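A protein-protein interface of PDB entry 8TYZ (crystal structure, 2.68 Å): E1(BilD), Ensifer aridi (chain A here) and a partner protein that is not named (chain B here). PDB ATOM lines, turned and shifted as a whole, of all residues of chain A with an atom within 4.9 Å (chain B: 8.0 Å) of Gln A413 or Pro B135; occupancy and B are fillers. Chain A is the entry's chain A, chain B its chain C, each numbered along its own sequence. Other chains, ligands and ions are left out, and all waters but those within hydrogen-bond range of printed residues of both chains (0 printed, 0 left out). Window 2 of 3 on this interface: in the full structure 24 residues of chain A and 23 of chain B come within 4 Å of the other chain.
ND2 of Asn B148 sits at hydrogen-bond distance from O of Cys A417. SG of Cys B138 is disulfide-bonded to SG of Cys A417 (2.0 Å). A ring nitrogen (ND1) of His B151 lies close to the side-chain hydroxyl (OH) of Tyr A412, 3.3 Å away. The side-chain sulfur (SG) of Cys A417 is in hydrogen-bond range of a ring nitrogen (NE2) of His B151, at 2.7 Å.
Among the printed residues, pairs that only touch across the chains: Gln A413 with Pro B135 and Ile A416 with Ala B150.
Gln A413 touches just one residue of chain B: Pro B135. Of chain A, only Gln A413 comes within 4 Å of Pro B135. Of the printed residues of chain A, Cys B138 touches Cys A417 (2.0 Å). Of the printed residues of chain B, Ile A416 touches Ala B150. Of the printed residues of chain A, Ala B150 touches Ile A416. Of the printed residues of chain B, Tyr A412 touches His B151 (2.9 Å). Gly A418 touches none of the printed residues of chain B. The nearest residue of chain B that does not touch Gln A413 is Ser B134 (4.1 Å). The nearest printed residue of chain A that does not touch Asn B148 is Ile A416 (4.9 Å).
Of the 11 printed residues of chain A, 4 touch a printed residue of chain B. Of the 11 printed residues of chain B, 5 touch a printed residue of chain A. Printed residues of chain B that touch a printed residue of chain A: Pro B135, Cys B138, Asn B148, Ala B150 and His B151. Hydrophobic or aromatic side chains of chain B that line the printed part of chain A: Pro B135, Ala B150 and His B151. Among the printed residues, 6 pairs touch across the chains. Among the printed residues, no Asp or Glu carboxylate lies within 4 Å of a Lys or Arg side-chain nitrogen of the other chain.
OD1 of Asn B148 sits at hydrogen-bond distance from N of Ala B150, 3.0 Å away. The backbone carbonyl oxygen (O) of Gln A413 is in hydrogen-bond range of the backbone NH (N) of Gly A418 (2.6 Å). The backbone carbonyl oxygen (O) of Tyr A412 lies within hydrogen-bond range of the backbone NH (N) of Cys A417. SG of Cys B138 sits at hydrogen-bond distance from NE2 of His B151, 2.6 Å away. N of Cys B138 is in hydrogen-bond range of OG of Ser B134.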
ATOM      1  N   LEU A 408      12.669   4.089 -16.205  1.00  0.00           N
ATOM      2  CA  LEU A 408      12.418   3.361 -17.440  1.00  0.00           C
ATOM      3  C   LEU A 408      11.663   2.074 -17.168  1.00  0.00           C
ATOM      4  O   LEU A 408      10.809   1.678 -17.969  1.00  0.00           O
ATOM      5  CB  LEU A 408      13.727   3.070 -18.168  1.00  0.00           C
ATOM      6  CG  LEU A 408      13.528   2.321 -19.496  1.00  0.00           C
ATOM      7  CD1 LEU A 408      12.445   2.956 -20.390  1.00  0.00           C
ATOM      8  CD2 LEU A 408      14.852   2.208 -20.257  1.00  0.00           C
ATOM      9  N   ARG A 409      11.943   1.421 -16.035  1.00  0.00           N
ATOM     10  CA  ARG A 409      11.261   0.169 -15.722  1.00  0.00           C
ATOM     11  C   ARG A 409       9.763   0.384 -15.564  1.00  0.00           C
ATOM     12  O   ARG A 409       8.965  -0.423 -16.055  1.00  0.00           O
ATOM     13  CB  ARG A 409      11.856  -0.455 -14.463  1.00  0.00           C
ATOM     14  CG  ARG A 409      13.352  -0.692 -14.526  1.00  0.00           C
ATOM     15  CD  ARG A 409      13.868  -1.389 -13.264  1.00  0.00           C
ATOM     16  NE  ARG A 409      15.324  -1.396 -13.243  1.00  0.00           N
ATOM     17  CZ  ARG A 409      16.071  -2.178 -14.012  1.00  0.00           C
ATOM     18  NH1 ARG A 409      15.525  -3.080 -14.816  1.00  0.00           N
ATOM     19  NH2 ARG A 409      17.397  -2.042 -13.983  1.00  0.00           N
ATOM     20  N   SER A 410       9.362   1.471 -14.889  1.00  0.00           N
ATOM     21  CA  SER A 410       7.937   1.745 -14.694  1.00  0.00           C
ATOM     22  C   SER A 410       7.250   1.975 -16.026  1.00  0.00           C
ATOM     23  O   SER A 410       6.149   1.458 -16.267  1.00  0.00           O
ATOM     24  CB  SER A 410       7.746   2.962 -13.792  1.00  0.00           C
ATOM     25  OG  SER A 410       8.670   2.942 -12.719  1.00  0.00           O
ATOM     26  N   PHE A 411       7.898   2.749 -16.903  1.00  0.00           N
ATOM     27  CA  PHE A 411       7.426   2.940 -18.272  1.00  0.00           C
ATOM     28  C   PHE A 411       7.310   1.601 -18.992  1.00  0.00           C
ATOM     29  O   PHE A 411       6.228   1.221 -19.459  1.00  0.00           O
ATOM     30  CB  PHE A 411       8.385   3.889 -19.000  1.00  0.00           C
ATOM     31  CG  PHE A 411       7.956   4.266 -20.395  1.00  0.00           C
ATOM     32  CD1 PHE A 411       6.621   4.444 -20.711  1.00  0.00           C
ATOM     33  CD2 PHE A 411       8.911   4.484 -21.389  1.00  0.00           C
ATOM     34  CE1 PHE A 411       6.239   4.802 -21.995  1.00  0.00           C
ATOM     35  CE2 PHE A 411       8.531   4.845 -22.679  1.00  0.00           C
ATOM     36  CZ  PHE A 411       7.193   5.001 -22.977  1.00  0.00           C
ATOM     37  N   TYR A 412       8.422   0.856 -19.064  1.00  0.00           N
ATOM     38  CA  TYR A 412       8.412  -0.414 -19.779  1.00  0.00           C
ATOM     39  C   TYR A 412       7.373  -1.357 -19.200  1.00  0.00           C
ATOM     40  O   TYR A 412       6.709  -2.090 -19.946  1.00  0.00           O
ATOM     41  CB  TYR A 412       9.789  -1.077 -19.752  1.00  0.00           C
ATOM     42  CG  TYR A 412       9.754  -2.506 -20.259  1.00  0.00           C
ATOM     43  CD1 TYR A 412       9.671  -3.575 -19.372  1.00  0.00           C
ATOM     44  CD2 TYR A 412       9.772  -2.787 -21.617  1.00  0.00           C
ATOM     45  CE1 TYR A 412       9.617  -4.886 -19.821  1.00  0.00           C
ATOM     46  CE2 TYR A 412       9.722  -4.103 -22.076  1.00  0.00           C
ATOM     47  CZ  TYR A 412       9.642  -5.150 -21.171  1.00  0.00           C
ATOM     48  OH  TYR A 412       9.596  -6.465 -21.591  1.00  0.00           O
ATOM     49  N   GLN A 413       7.207  -1.343 -17.869  1.00  0.00           N
ATOM     50  CA  GLN A 413       6.263  -2.257 -17.245  1.00  0.00           C
ATOM     51  C   GLN A 413       4.847  -1.987 -17.724  1.00  0.00           C
ATOM     52  O   GLN A 413       4.143  -2.910 -18.151  1.00  0.00           O
ATOM     53  CB  GLN A 413       6.340  -2.165 -15.729  1.00  0.00           C
ATOM     54  CG  GLN A 413       5.491  -3.245 -15.054  1.00  0.00           C
ATOM     55  CD  GLN A 413       5.961  -3.582 -13.649  1.00  0.00           C
ATOM     56  OE1 GLN A 413       6.867  -2.934 -13.104  1.00  0.00           O
ATOM     57  NE2 GLN A 413       5.345  -4.608 -13.050  1.00  0.00           N
ATOM     58  N   GLN A 414       4.422  -0.717 -17.698  1.00  0.00           N
ATOM     59  CA  GLN A 414       3.023  -0.404 -18.002  1.00  0.00           C
ATOM     60  C   GLN A 414       2.745  -0.310 -19.505  1.00  0.00           C
ATOM     61  O   GLN A 414       1.658  -0.706 -19.951  1.00  0.00           O
ATOM     62  CB  GLN A 414       2.608   0.886 -17.286  1.00  0.00           C
ATOM     63  CG  GLN A 414       3.000   0.884 -15.814  1.00  0.00           C
ATOM     64  CD  GLN A 414       2.512   2.108 -15.041  1.00  0.00           C
ATOM     65  OE1 GLN A 414       1.359   2.533 -15.197  1.00  0.00           O
ATOM     66  NE2 GLN A 414       3.391   2.675 -14.191  1.00  0.00           N
ATOM     67  N   ALA A 415       3.700   0.178 -20.306  1.00  0.00           N
ATOM     68  CA  ALA A 415       3.445   0.281 -21.741  1.00  0.00           C
ATOM     69  C   ALA A 415       3.613  -1.062 -22.450  1.00  0.00           C
ATOM     70  O   ALA A 415       2.865  -1.367 -23.388  1.00  0.00           O
ATOM     71  CB  ALA A 415       4.361   1.330 -22.366  1.00  0.00           C
ATOM     72  N   ILE A 416       4.583  -1.877 -22.027  1.00  0.00           N
ATOM     73  CA  ILE A 416       4.767  -3.195 -22.632  1.00  0.00           C
ATOM     74  C   ILE A 416       4.103  -4.283 -21.798  1.00  0.00           C
ATOM     75  O   ILE A 416       3.063  -4.811 -22.204  1.00  0.00           O
ATOM     76  CB  ILE A 416       6.251  -3.524 -22.856  1.00  0.00           C
ATOM     77  CG1 ILE A 416       6.911  -2.417 -23.669  1.00  0.00           C
ATOM     78  CG2 ILE A 416       6.380  -4.864 -23.577  1.00  0.00           C
ATOM     79  CD1 ILE A 416       6.193  -2.153 -24.939  1.00  0.00           C
ATOM     80  N   CYS A 417       4.701  -4.641 -20.639  1.00  0.00           N
ATOM     81  CA  CYS A 417       4.176  -5.789 -19.893  1.00  0.00           C
ATOM     82  C   CYS A 417       2.699  -5.575 -19.566  1.00  0.00           C
ATOM     83  O   CYS A 417       1.896  -6.512 -19.690  1.00  0.00           O
ATOM     84  CB  CYS A 417       5.011  -6.099 -18.622  1.00  0.00           C
ATOM     85  SG  CYS A 417       4.982  -7.946 -18.132  1.00  0.00           S
ATOM     86  N   GLY A 418       2.299  -4.328 -19.287  1.00  0.00           N
ATOM     87  CA  GLY A 418       0.905  -4.023 -19.028  1.00  0.00           C
ATOM     88  C   GLY A 418      -0.006  -3.953 -20.243  1.00  0.00           C
ATOM     89  O   GLY A 418      -1.227  -3.892 -20.091  1.00  0.00           O
ATOM     90  N   PHE B  79       1.231 -16.635  -6.273  1.00  0.00           N
ATOM     91  CA  PHE B  79       1.170 -16.224  -4.877  1.00  0.00           C
ATOM     92  C   PHE B  79      -0.133 -16.728  -4.273  1.00  0.00           C
ATOM     93  O   PHE B  79      -1.223 -16.387  -4.748  1.00  0.00           O
ATOM     94  CB  PHE B  79       1.305 -14.710  -4.754  1.00  0.00           C
ATOM     95  CG  PHE B  79       2.637 -14.207  -5.205  1.00  0.00           C
ATOM     96  CD1 PHE B  79       2.887 -13.994  -6.559  1.00  0.00           C
ATOM     97  CD2 PHE B  79       3.662 -13.988  -4.293  1.00  0.00           C
ATOM     98  CE1 PHE B  79       4.139 -13.545  -7.005  1.00  0.00           C
ATOM     99  CE2 PHE B  79       4.916 -13.540  -4.724  1.00  0.00           C
ATOM    100  CZ  PHE B  79       5.156 -13.318  -6.084  1.00  0.00           C
ATOM    101  N   SER B 134      10.099  -7.012 -10.858  1.00  0.00           N
ATOM    102  CA  SER B 134       8.781  -6.663 -11.391  1.00  0.00           C
ATOM    103  C   SER B 134       7.664  -7.352 -10.599  1.00  0.00           C
ATOM    104  O   SER B 134       7.702  -8.581 -10.410  1.00  0.00           O
ATOM    105  CB  SER B 134       8.674  -7.047 -12.872  1.00  0.00           C
ATOM    106  OG  SER B 134       8.490  -8.448 -13.028  1.00  0.00           O
ATOM    107  N   PRO B 135       6.682  -6.565 -10.133  1.00  0.00           N
ATOM    108  CA  PRO B 135       5.524  -7.155  -9.427  1.00  0.00           C
ATOM    109  C   PRO B 135       4.703  -8.077 -10.329  1.00  0.00           C
ATOM    110  O   PRO B 135       4.415  -7.748 -11.488  1.00  0.00           O
ATOM    111  CB  PRO B 135       4.705  -5.930  -8.986  1.00  0.00           C
ATOM    112  CG  PRO B 135       5.689  -4.742  -9.036  1.00  0.00           C
ATOM    113  CD  PRO B 135       6.678  -5.085 -10.121  1.00  0.00           C
ATOM    114  N   PHE B 136       4.322  -9.236  -9.763  1.00  0.00           N
ATOM    115  CA  PHE B 136       3.598 -10.379 -10.346  1.00  0.00           C
ATOM    116  C   PHE B 136       4.560 -11.418 -10.931  1.00  0.00           C
ATOM    117  O   PHE B 136       4.163 -12.579 -11.106  1.00  0.00           O
ATOM    118  CB  PHE B 136       2.559  -9.971 -11.415  1.00  0.00           C
ATOM    119  CG  PHE B 136       1.830 -11.128 -12.053  1.00  0.00           C
ATOM    120  CD1 PHE B 136       1.105 -12.045 -11.267  1.00  0.00           C
ATOM    121  CD2 PHE B 136       1.862 -11.301 -13.438  1.00  0.00           C
ATOM    122  CE1 PHE B 136       0.428 -13.122 -11.861  1.00  0.00           C
ATOM    123  CE2 PHE B 136       1.193 -12.367 -14.041  1.00  0.00           C
ATOM    124  CZ  PHE B 136       0.471 -13.278 -13.257  1.00  0.00           C
ATOM    125  N   LEU B 137       5.825 -11.032 -11.193  1.00  0.00           N
ATOM    126  CA  LEU B 137       6.913 -11.829 -11.770  1.00  0.00           C
ATOM    127  C   LEU B 137       6.867 -11.883 -13.291  1.00  0.00           C
ATOM    128  O   LEU B 137       6.889 -12.970 -13.874  1.00  0.00           O
ATOM    129  CB  LEU B 137       6.940 -13.257 -11.213  1.00  0.00           C
ATOM    130  CG  LEU B 137       7.604 -13.298  -9.840  1.00  0.00           C
ATOM    131  CD1 LEU B 137       7.760 -14.724  -9.381  1.00  0.00           C
ATOM    132  CD2 LEU B 137       8.944 -12.609  -9.916  1.00  0.00           C
ATOM    133  N   CYS B 138       6.832 -10.726 -13.946  1.00  0.00           N
ATOM    134  CA  CYS B 138       7.036 -10.657 -15.391  1.00  0.00           C
ATOM    135  C   CYS B 138       8.547 -10.726 -15.601  1.00  0.00           C
ATOM    136  O   CYS B 138       9.240  -9.716 -15.739  1.00  0.00           O
ATOM    137  CB  CYS B 138       6.373  -9.389 -15.953  1.00  0.00           C
ATOM    138  SG  CYS B 138       6.812  -8.543 -17.552  1.00  0.00           S
ATOM    139  N   MET B 139       9.074 -11.944 -15.557  1.00  0.00           N
ATOM    140  CA  MET B 139      10.473 -12.178 -15.871  1.00  0.00           C
ATOM    141  C   MET B 139      10.604 -13.473 -16.651  1.00  0.00           C
ATOM    142  O   MET B 139       9.833 -14.417 -16.460  1.00  0.00           O
ATOM    143  CB  MET B 139      11.350 -12.243 -14.619  1.00  0.00           C
ATOM    144  CG  MET B 139      11.053 -13.412 -13.703  1.00  0.00           C
ATOM    145  SD  MET B 139      12.315 -13.657 -12.437  1.00  0.00           S
ATOM    146  CE  MET B 139      11.405 -14.680 -11.274  1.00  0.00           C
ATOM    147  N   ASN B 148       2.214 -13.926 -21.633  1.00  0.00           N
ATOM    148  CA  ASN B 148       1.822 -12.555 -21.952  1.00  0.00           C
ATOM    149  C   ASN B 148       2.120 -12.297 -23.424  1.00  0.00           C
ATOM    150  O   ASN B 148       3.266 -12.496 -23.864  1.00  0.00           O
ATOM    151  CB  ASN B 148       2.583 -11.569 -21.061  1.00  0.00           C
ATOM    152  CG  ASN B 148       2.074 -10.145 -21.176  1.00  0.00           C
ATOM    153  OD1 ASN B 148       1.321  -9.801 -22.081  1.00  0.00           O
ATOM    154  ND2 ASN B 148       2.492  -9.305 -20.246  1.00  0.00           N
ATOM    155  N   ALA B 150       2.491  -9.471 -24.857  1.00  0.00           N
ATOM    156  CA  ALA B 150       3.467  -8.387 -24.930  1.00  0.00           C
ATOM    157  C   ALA B 150       4.902  -8.903 -24.883  1.00  0.00           C
ATOM    158  O   ALA B 150       5.834  -8.198 -25.293  1.00  0.00           O
ATOM    159  CB  ALA B 150       3.223  -7.407 -23.790  1.00  0.00           C
ATOM    160  N   HIS B 151       5.103 -10.114 -24.368  1.00  0.00           N
ATOM    161  CA  HIS B 151       6.409 -10.752 -24.314  1.00  0.00           C
ATOM    162  C   HIS B 151       6.528 -11.882 -25.334  1.00  0.00           C
ATOM    163  O   HIS B 151       7.380 -12.767 -25.184  1.00  0.00           O
ATOM    164  CB  HIS B 151       6.690 -11.270 -22.899  1.00  0.00           C
ATOM    165  CG  HIS B 151       6.778 -10.196 -21.854  1.00  0.00           C
ATOM    166  ND1 HIS B 151       7.666  -9.142 -21.935  1.00  0.00           N
ATOM    167  CD2 HIS B 151       6.100 -10.029 -20.691  1.00  0.00           C
ATOM    168  CE1 HIS B 151       7.521  -8.368 -20.871  1.00  0.00           C
ATOM    169  NE2 HIS B 151       6.584  -8.888 -20.095  1.00  0.00           N
ATOM    170  N   TYR B 177      14.543  -9.009  -4.448  1.00  0.00           N
ATOM    171  CA  TYR B 177      13.701  -7.818  -4.509  1.00  0.00           C
ATOM    172  C   TYR B 177      12.624  -7.813  -3.431  1.00  0.00           C
ATOM    173  O   TYR B 177      12.075  -6.746  -3.122  1.00  0.00           O
ATOM    174  CB  TYR B 177      13.054  -7.686  -5.887  1.00  0.00           C
ATOM    175  CG  TYR B 177      14.036  -7.739  -7.045  1.00  0.00           C
ATOM    176  CD1 TYR B 177      14.805  -6.621  -7.400  1.00  0.00           C
ATOM    177  CD2 TYR B 177      14.190  -8.913  -7.793  1.00  0.00           C
ATOM    178  CE1 TYR B 177      15.704  -6.676  -8.473  1.00  0.00           C
ATOM    179  CE2 TYR B 177      15.081  -8.982  -8.857  1.00  0.00           C
ATOM    180  CZ  TYR B 177      15.833  -7.863  -9.195  1.00  0.00           C
ATOM    181  OH  TYR B 177      16.712  -7.934 -10.252  1.00  0.00           O
